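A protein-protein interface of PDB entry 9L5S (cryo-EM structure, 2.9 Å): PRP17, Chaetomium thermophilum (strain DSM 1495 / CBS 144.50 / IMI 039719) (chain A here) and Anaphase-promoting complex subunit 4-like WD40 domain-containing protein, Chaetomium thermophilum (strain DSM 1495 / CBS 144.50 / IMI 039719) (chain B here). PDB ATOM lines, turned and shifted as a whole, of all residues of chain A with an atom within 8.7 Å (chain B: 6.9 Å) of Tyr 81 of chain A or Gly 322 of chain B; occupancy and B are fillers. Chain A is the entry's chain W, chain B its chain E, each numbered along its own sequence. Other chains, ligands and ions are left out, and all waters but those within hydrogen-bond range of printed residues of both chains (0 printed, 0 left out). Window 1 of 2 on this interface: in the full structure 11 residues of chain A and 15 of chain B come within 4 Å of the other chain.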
ATOM      1  N   GLU A  78      18.799 -19.389  12.968  1.00  0.00           N
ATOM      2  CA  GLU A  78      18.655 -18.608  11.750  1.00  0.00           C
ATOM      3  C   GLU A  78      17.635 -19.271  10.837  1.00  0.00           C
ATOM      4  O   GLU A  78      17.418 -20.484  10.900  1.00  0.00           O
ATOM      5  CB  GLU A  78      19.996 -18.456  11.012  1.00  0.00           C
ATOM      6  CG  GLU A  78      20.565 -19.760  10.474  1.00  0.00           C
ATOM      7  CD  GLU A  78      21.915 -19.580   9.811  1.00  0.00           C
ATOM      8  OE1 GLU A  78      22.423 -18.440   9.790  1.00  0.00           O
ATOM      9  OE2 GLU A  78      22.466 -20.580   9.304  1.00  0.00           O
ATOM     10  N   GLU A  79      16.999 -18.461   9.995  1.00  0.00           N
ATOM     11  CA  GLU A  79      16.066 -18.998   9.015  1.00  0.00           C
ATOM     12  C   GLU A  79      16.830 -19.608   7.848  1.00  0.00           C
ATOM     13  O   GLU A  79      17.761 -19.004   7.310  1.00  0.00           O
ATOM     14  CB  GLU A  79      15.124 -17.904   8.514  1.00  0.00           C
ATOM     15  CG  GLU A  79      13.765 -18.419   8.066  1.00  0.00           C
ATOM     16  CD  GLU A  79      13.011 -17.414   7.217  1.00  0.00           C
ATOM     17  OE1 GLU A  79      11.944 -17.772   6.675  1.00  0.00           O
ATOM     18  OE2 GLU A  79      13.488 -16.268   7.086  1.00  0.00           O
ATOM     19  N   MET A  80      16.431 -20.813   7.456  1.00  0.00           N
ATOM     20  CA  MET A  80      17.110 -21.545   6.401  1.00  0.00           C
ATOM     21  C   MET A  80      16.081 -22.042   5.397  1.00  0.00           C
ATOM     22  O   MET A  80      14.882 -22.109   5.681  1.00  0.00           O
ATOM     23  CB  MET A  80      17.922 -22.711   6.977  1.00  0.00           C
ATOM     24  CG  MET A  80      17.156 -24.008   7.117  1.00  0.00           C
ATOM     25  SD  MET A  80      18.114 -25.216   8.037  1.00  0.00           S
ATOM     26  CE  MET A  80      19.289 -25.761   6.806  1.00  0.00           C
ATOM     27  N   TYR A  81      16.559 -22.383   4.204  1.00  0.00           N
ATOM     28  CA  TYR A  81      15.698 -22.844   3.116  1.00  0.00           C
ATOM     29  C   TYR A  81      16.250 -24.160   2.581  1.00  0.00           C
ATOM     30  O   TYR A  81      17.332 -24.192   1.988  1.00  0.00           O
ATOM     31  CB  TYR A  81      15.607 -21.800   2.015  1.00  0.00           C
ATOM     32  CG  TYR A  81      14.683 -20.647   2.326  1.00  0.00           C
ATOM     33  CD1 TYR A  81      15.089 -19.610   3.156  1.00  0.00           C
ATOM     34  CD2 TYR A  81      13.412 -20.585   1.773  1.00  0.00           C
ATOM     35  CE1 TYR A  81      14.250 -18.550   3.436  1.00  0.00           C
ATOM     36  CE2 TYR A  81      12.565 -19.530   2.045  1.00  0.00           C
ATOM     37  CZ  TYR A  81      12.989 -18.516   2.877  1.00  0.00           C
ATOM     38  OH  TYR A  81      12.145 -17.465   3.149  1.00  0.00           O
ATOM     39  N   ILE A  82      15.507 -25.242   2.798  1.00  0.00           N
ATOM     40  CA  ILE A  82      15.828 -26.548   2.245  1.00  0.00           C
ATOM     41  C   ILE A  82      14.571 -27.135   1.625  1.00  0.00           C
ATOM     42  O   ILE A  82      13.452 -26.676   1.866  1.00  0.00           O
ATOM     43  CB  ILE A  82      16.408 -27.525   3.289  1.00  0.00           C
ATOM     44  CG1 ILE A  82      15.413 -27.743   4.433  1.00  0.00           C
ATOM     45  CG2 ILE A  82      17.769 -27.068   3.770  1.00  0.00           C
ATOM     46  CD1 ILE A  82      15.806 -28.849   5.379  1.00  0.00           C
ATOM     47  N   SER A  83      14.775 -28.160   0.805  1.00  0.00           N
ATOM     48  CA  SER A  83      13.659 -28.896   0.243  1.00  0.00           C
ATOM     49  C   SER A  83      12.928 -29.668   1.337  1.00  0.00           C
ATOM     50  O   SER A  83      13.496 -30.016   2.376  1.00  0.00           O
ATOM     51  CB  SER A  83      14.142 -29.852  -0.847  1.00  0.00           C
ATOM     52  OG  SER A  83      14.880 -30.924  -0.292  1.00  0.00           O
ATOM     53  N   GLU A  84      11.637 -29.908   1.097  1.00  0.00           N
ATOM     54  CA  GLU A  84      10.842 -30.716   2.018  1.00  0.00           C
ATOM     55  C   GLU A  84      11.369 -32.144   2.086  1.00  0.00           C
ATOM     56  O   GLU A  84      11.396 -32.757   3.161  1.00  0.00           O
ATOM     57  CB  GLU A  84       9.379 -30.703   1.581  1.00  0.00           C
ATOM     58  CG  GLU A  84       8.406 -31.281   2.591  1.00  0.00           C
ATOM     59  CD  GLU A  84       8.363 -30.492   3.882  1.00  0.00           C
ATOM     60  OE1 GLU A  84       8.437 -29.247   3.825  1.00  0.00           O
ATOM     61  OE2 GLU A  84       8.250 -31.119   4.957  1.00  0.00           O
ATOM     62  N   THR A  86      14.430 -33.237   1.740  1.00  0.00           N
ATOM     63  CA  THR A  86      15.660 -33.350   2.522  1.00  0.00           C
ATOM     64  C   THR A  86      15.360 -33.492   4.009  1.00  0.00           C
ATOM     65  O   THR A  86      15.900 -34.382   4.684  1.00  0.00           O
ATOM     66  CB  THR A  86      16.553 -32.133   2.272  1.00  0.00           C
ATOM     67  OG1 THR A  86      16.839 -32.024   0.873  1.00  0.00           O
ATOM     68  CG2 THR A  86      17.856 -32.255   3.041  1.00  0.00           C
ATOM     69  N   GLU B  62      12.249 -23.891  -5.215  1.00  0.00           N
ATOM     70  CA  GLU B  62      13.701 -23.789  -5.243  1.00  0.00           C
ATOM     71  C   GLU B  62      14.183 -23.551  -6.665  1.00  0.00           C
ATOM     72  O   GLU B  62      13.861 -24.322  -7.574  1.00  0.00           O
ATOM     73  CB  GLU B  62      14.312 -25.073  -4.690  1.00  0.00           C
ATOM     74  CG  GLU B  62      13.990 -25.312  -3.232  1.00  0.00           C
ATOM     75  CD  GLU B  62      12.774 -26.202  -3.062  1.00  0.00           C
ATOM     76  OE1 GLU B  62      11.669 -25.780  -3.465  1.00  0.00           O
ATOM     77  OE2 GLU B  62      12.921 -27.323  -2.542  1.00  0.00           O
ATOM     78  N   GLU B 279      21.811 -30.307   1.856  1.00  0.00           N
ATOM     79  CA  GLU B 279      21.151 -30.671   0.613  1.00  0.00           C
ATOM     80  C   GLU B 279      22.148 -31.251  -0.380  1.00  0.00           C
ATOM     81  O   GLU B 279      23.243 -30.714  -0.571  1.00  0.00           O
ATOM     82  CB  GLU B 279      20.461 -29.455  -0.007  1.00  0.00           C
ATOM     83  CG  GLU B 279      19.041 -29.225   0.473  1.00  0.00           C
ATOM     84  CD  GLU B 279      18.485 -27.895   0.008  1.00  0.00           C
ATOM     85  OE1 GLU B 279      19.220 -26.888   0.066  1.00  0.00           O
ATOM     86  OE2 GLU B 279      17.317 -27.862  -0.432  1.00  0.00           O
ATOM     87  N   ASN B 281      22.198 -31.137  -3.641  1.00  0.00           N
ATOM     88  CA  ASN B 281      21.776 -30.493  -4.873  1.00  0.00           C
ATOM     89  C   ASN B 281      22.854 -30.621  -5.947  1.00  0.00           C
ATOM     90  O   ASN B 281      24.002 -30.984  -5.681  1.00  0.00           O
ATOM     91  CB  ASN B 281      21.459 -29.020  -4.627  1.00  0.00           C
ATOM     92  CG  ASN B 281      20.077 -28.809  -4.053  1.00  0.00           C
ATOM     93  OD1 ASN B 281      19.123 -29.478  -4.445  1.00  0.00           O
ATOM     94  ND2 ASN B 281      19.960 -27.874  -3.120  1.00  0.00           N
ATOM     95  N   ALA B 298      27.910 -22.328  -2.878  1.00  0.00           N
ATOM     96  CA  ALA B 298      28.136 -23.127  -1.684  1.00  0.00           C
ATOM     97  C   ALA B 298      26.822 -23.379  -0.956  1.00  0.00           C
ATOM     98  O   ALA B 298      25.795 -22.757  -1.237  1.00  0.00           O
ATOM     99  CB  ALA B 298      29.141 -22.444  -0.750  1.00  0.00           C
ATOM    100  N   GLY B 299      26.871 -24.311  -0.008  1.00  0.00           N
ATOM    101  CA  GLY B 299      25.734 -24.616   0.832  1.00  0.00           C
ATOM    102  C   GLY B 299      25.508 -23.662   1.978  1.00  0.00           C
ATOM    103  O   GLY B 299      24.518 -23.798   2.703  1.00  0.00           O
ATOM    104  N   ASP B 300      26.401 -22.694   2.165  1.00  0.00           N
ATOM    105  CA  ASP B 300      26.272 -21.682   3.203  1.00  0.00           C
ATOM    106  C   ASP B 300      25.537 -20.441   2.720  1.00  0.00           C
ATOM    107  O   ASP B 300      25.465 -19.452   3.456  1.00  0.00           O
ATOM    108  CB  ASP B 300      27.655 -21.282   3.725  1.00  0.00           C
ATOM    109  CG  ASP B 300      28.431 -22.455   4.283  1.00  0.00           C
ATOM    110  OD1 ASP B 300      27.830 -23.531   4.480  1.00  0.00           O
ATOM    111  OD2 ASP B 300      29.646 -22.299   4.528  1.00  0.00           O
ATOM    112  N   GLY B 301      24.996 -20.468   1.506  1.00  0.00           N
ATOM    113  CA  GLY B 301      24.438 -19.275   0.912  1.00  0.00           C
ATOM    114  C   GLY B 301      25.452 -18.369   0.259  1.00  0.00           C
ATOM    115  O   GLY B 301      25.093 -17.266  -0.167  1.00  0.00           O
ATOM    116  N   THR B 302      26.706 -18.799   0.168  1.00  0.00           N
ATOM    117  CA  THR B 302      27.780 -18.002  -0.396  1.00  0.00           C
ATOM    118  C   THR B 302      28.156 -18.515  -1.780  1.00  0.00           C
ATOM    119  O   THR B 302      27.938 -19.681  -2.121  1.00  0.00           O
ATOM    120  CB  THR B 302      29.016 -18.024   0.509  1.00  0.00           C
ATOM    121  OG1 THR B 302      29.486 -19.370   0.642  1.00  0.00           O
ATOM    122  CG2 THR B 302      28.680 -17.478   1.885  1.00  0.00           C
ATOM    123  N   GLY B 319      24.655 -13.766   1.285  1.00  0.00           N
ATOM    124  CA  GLY B 319      23.412 -13.126   0.890  1.00  0.00           C
ATOM    125  C   GLY B 319      22.269 -14.073   0.600  1.00  0.00           C
ATOM    126  O   GLY B 319      21.174 -13.605   0.259  1.00  0.00           O
ATOM    127  N   HIS B 320      22.464 -15.382   0.712  1.00  0.00           N
ATOM    128  CA  HIS B 320      21.416 -16.356   0.461  1.00  0.00           C
ATOM    129  C   HIS B 320      21.167 -17.170   1.723  1.00  0.00           C
ATOM    130  O   HIS B 320      22.082 -17.410   2.516  1.00  0.00           O
ATOM    131  CB  HIS B 320      21.791 -17.286  -0.697  1.00  0.00           C
ATOM    132  CG  HIS B 320      21.785 -16.618  -2.035  1.00  0.00           C
ATOM    133  ND1 HIS B 320      20.625 -16.227  -2.668  1.00  0.00           N
ATOM    134  CD2 HIS B 320      22.800 -16.270  -2.862  1.00  0.00           C
ATOM    135  CE1 HIS B 320      20.924 -15.670  -3.827  1.00  0.00           C
ATOM    136  NE2 HIS B 320      22.237 -15.682  -3.968  1.00  0.00           N
ATOM    137  N   LYS B 321      19.920 -17.594   1.901  1.00  0.00           N
ATOM    138  CA  LYS B 321      19.506 -18.378   3.059  1.00  0.00           C
ATOM    139  C   LYS B 321      19.289 -19.840   2.684  1.00  0.00           C
ATOM    140  O   LYS B 321      18.544 -20.567   3.342  1.00  0.00           O
ATOM    141  CB  LYS B 321      18.247 -17.789   3.688  1.00  0.00           C
ATOM    142  CG  LYS B 321      18.364 -16.314   4.026  1.00  0.00           C
ATOM    143  CD  LYS B 321      17.586 -15.974   5.284  1.00  0.00           C
ATOM    144  CE  LYS B 321      17.549 -14.473   5.522  1.00  0.00           C
ATOM    145  NZ  LYS B 321      16.344 -13.841   4.918  1.00  0.00           N
ATOM    146  N   GLY B 322      19.945 -20.281   1.620  1.00  0.00           N
ATOM    147  CA  GLY B 322      19.840 -21.659   1.181  1.00  0.00           C
ATOM    148  C   GLY B 322      21.024 -21.998   0.307  1.00  0.00           C
ATOM    149  O   GLY B 322      21.902 -21.164   0.060  1.00  0.00           O
ATOM    150  N   THR B 323      21.041 -23.246  -0.154  1.00  0.00           N
ATOM    151  CA  THR B 323      22.110 -23.717  -1.025  1.00  0.00           C
ATOM    152  C   THR B 323      22.058 -23.001  -2.367  1.00  0.00           C
ATOM    153  O   THR B 323      21.037 -23.027  -3.059  1.00  0.00           O
ATOM    154  CB  THR B 323      21.995 -25.231  -1.224  1.00  0.00           C
ATOM    155  OG1 THR B 323      22.295 -25.899   0.007  1.00  0.00           O
ATOM    156  CG2 THR B 323      22.960 -25.709  -2.295  1.00  0.00           C
ATOM    157  N   VAL B 324      23.165 -22.355  -2.729  1.00  0.00           N
ATOM    158  CA  VAL B 324      23.255 -21.636  -3.995  1.00  0.00           C
ATOM    159  C   VAL B 324      23.382 -22.674  -5.103  1.00  0.00           C
ATOM    160  O   VAL B 324      24.427 -23.309  -5.259  1.00  0.00           O
ATOM    161  CB  VAL B 324      24.436 -20.659  -4.009  1.00  0.00           C
ATOM    162  CG1 VAL B 324      24.533 -19.963  -5.357  1.00  0.00           C
ATOM    163  CG2 VAL B 324      24.294 -19.643  -2.894  1.00  0.00           C
ATOM    164  N   ASN B 325      22.309 -22.851  -5.875  1.00  0.00           N
ATOM    165  CA  ASN B 325      22.294 -23.895  -6.891  1.00  0.00           C
ATOM    166  C   ASN B 325      23.101 -23.514  -8.121  1.00  0.00           C
ATOM    167  O   ASN B 325      23.709 -24.390  -8.748  1.00  0.00           O
ATOM    168  CB  ASN B 325      20.854 -24.222  -7.288  1.00  0.00           C
ATOM    169  CG  ASN B 325      20.112 -24.988  -6.211  1.00  0.00           C
ATOM    170  OD1 ASN B 325      20.601 -25.996  -5.704  1.00  0.00           O
ATOM    171  ND2 ASN B 325      18.923 -24.514  -5.858  1.00  0.00           N
ATOM    172  N   SER B 341      19.506 -19.506  -5.900  1.00  0.00           N
ATOM    173  CA  SER B 341      19.541 -20.292  -4.679  1.00  0.00           C
ATOM    174  C   SER B 341      18.132 -20.688  -4.260  1.00  0.00           C
ATOM    175  O   SER B 341      17.142 -19.977  -4.518  1.00  0.00           O
ATOM    176  CB  SER B 341      20.228 -19.526  -3.545  1.00  0.00           C
ATOM    177  OG  SER B 341      19.529 -18.330  -3.266  1.00  0.00           O
ATOM    178  N   SER B 342      18.094 -21.804  -3.520  1.00  0.00           N
ATOM    179  CA  SER B 342      16.917 -22.519  -3.044  1.00  0.00           C
ATOM    180  C   SER B 342      16.173 -21.791  -1.936  1.00  0.00           C
ATOM    181  O   SER B 342      15.219 -22.350  -1.385  1.00  0.00           O
ATOM    182  CB  SER B 342      17.317 -23.916  -2.560  1.00  0.00           C
ATOM    183  OG  SER B 342      18.123 -23.847  -1.398  1.00  0.00           O
ATOM    184  N   ASP B 343      16.574 -20.566  -1.599  1.00  0.00           N
ATOM    185  CA  ASP B 343      15.692 -19.634  -0.918  1.00  0.00           C
ATOM    186  C   ASP B 343      14.807 -18.881  -1.903  1.00  0.00           C
ATOM    187  O   ASP B 343      14.391 -17.752  -1.616  1.00  0.00           O
ATOM    188  CB  ASP B 343      16.497 -18.673  -0.034  1.00  0.00           C
ATOM    189  CG  ASP B 343      17.515 -17.850  -0.806  1.00  0.00           C
ATOM    190  OD1 ASP B 343      17.663 -18.033  -2.031  1.00  0.00           O
ATOM    191  OD2 ASP B 343      18.176 -17.001  -0.174  1.00  0.00           O
ATOM    192  N   ARG B 344      14.566 -19.483  -3.072  1.00  0.00           N
ATOM    193  CA  ARG B 344      13.666 -19.022  -4.123  1.00  0.00           C
ATOM    194  C   ARG B 344      14.142 -17.729  -4.765  1.00  0.00           C
ATOM    195  O   ARG B 344      13.336 -17.000  -5.351  1.00  0.00           O
ATOM    196  CB  ARG B 344      12.231 -18.860  -3.601  1.00  0.00           C
ATOM    197  CG  ARG B 344      11.661 -20.112  -2.952  1.00  0.00           C
ATOM    198  CD  ARG B 344      10.279 -19.859  -2.383  1.00  0.00           C
ATOM    199  NE  ARG B 344       9.592 -21.098  -2.042  1.00  0.00           N
ATOM    200  CZ  ARG B 344       9.520 -21.601  -0.817  1.00  0.00           C
ATOM    201  NH1 ARG B 344      10.083 -20.994   0.213  1.00  0.00           N
ATOM    202  NH2 ARG B 344       8.865 -22.742  -0.623  1.00  0.00           N
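ND2 of Asn 281 of chain B sits at hydrogen-bond distance from OE1 of Glu 279 of chain B, 3.4 Å away. The backbone NH (N) of Gly 301 of chain B sits close to the backbone carbonyl oxygen (O) of Gly 322 of chain B, 3.5 Å away. The side-chain carboxylate (OE1) of Glu 279 of chain B is in hydrogen-bond range of the side-chain hydroxyl (OG1) of Thr 323 of chain B. The backbone NH of Ser 342 of chain B is in hydrogen-bond range of the backbone carbonyl oxygen of Thr 323 of chain B (3.2 Å). The backbone NH of Lys 321 of chain B sits at hydrogen-bond distance from the side-chain carboxylate of Asp 343 of chain B (2.8 Å). OG1 of Thr 86 of chain A is in hydrogen-bond range of OG of Ser 83 of chain A.
Of the printed residues of chain B, Met 80 of chain A touches Lys 321. Of the printed residues of chain B, Ile 82 of chain A touches Glu 279. Printed residues of chain B within 4 Å of Thr 86 of chain A: Glu 279. Of the printed residues of chain A, Lys 321 of chain B touches Glu 79 (3.6 Å), Met 80 (3.5 Å) and Tyr 81 (2.8 Å). Gly 322 of chain B touches just one residue of chain A: Tyr 81 (3.7 Å). Of the printed residues of chain A, Asp 343 of chain B touches Tyr 81. The nearest printed residue of chain A that does not touch Glu 279 of chain B is Glu 84 of chain A (6.2 Å).
The backbone NH (N) of Ser 83 of chain A lies within hydrogen-bond range of the side-chain carboxylate (OE2) of Glu 279 of chain B (2.8 Å). OG of Ser 342 of chain B is in hydrogen-bond range of O of Tyr 81 of chain A (3.5 Å). The backbone NH (N) of Tyr 81 of chain A sits at hydrogen-bond distance from the backbone carbonyl oxygen (O) of Lys 321 of chain B (2.8 Å).
Glu 79 of chain A touches Lys 321 of chain B. Lys 321 of chain B touches Met 80 of chain A (O to CA, 3.5 Å). O of Tyr 81 of chain A touches OE1 of Glu 279 of chain B, at 3.8 Å. Tyr 81 of chain A touches Gly 322 of chain B. Tyr 81 of chain A touches Asp 343 of chain B (CG to CA, 3.5 Å). Tyr 81 of chain A touches Arg 344 of chain B (CE2 to NH1, 3.4 Å). Glu 279 of chain B touches Ile 82 of chain A (OE2 to CA, 3.3 Å). OE2 of Glu 62 of chain B touches CB of Ser 83 of chain A (3.3 Å). Glu 279 of chain B touches Thr 86 of chain A.
Of the 8 printed residues of chain A, 6 touch a printed residue of chain B. Printed residues of chain A that touch a printed residue of chain B: Glu 79, Met 80, Tyr 81, Ile 82, Ser 83 and Thr 86. Printed residues of chain B that touch a printed residue of chain A: Glu 62, Glu 279, Lys 321, Gly 322, Ser 342, Asp 343 and Arg 344. Along chain B the printed residues that touch a printed residue of chain A span positions 62 to 344. Among the printed residues, 12 pairs touch across the chains.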
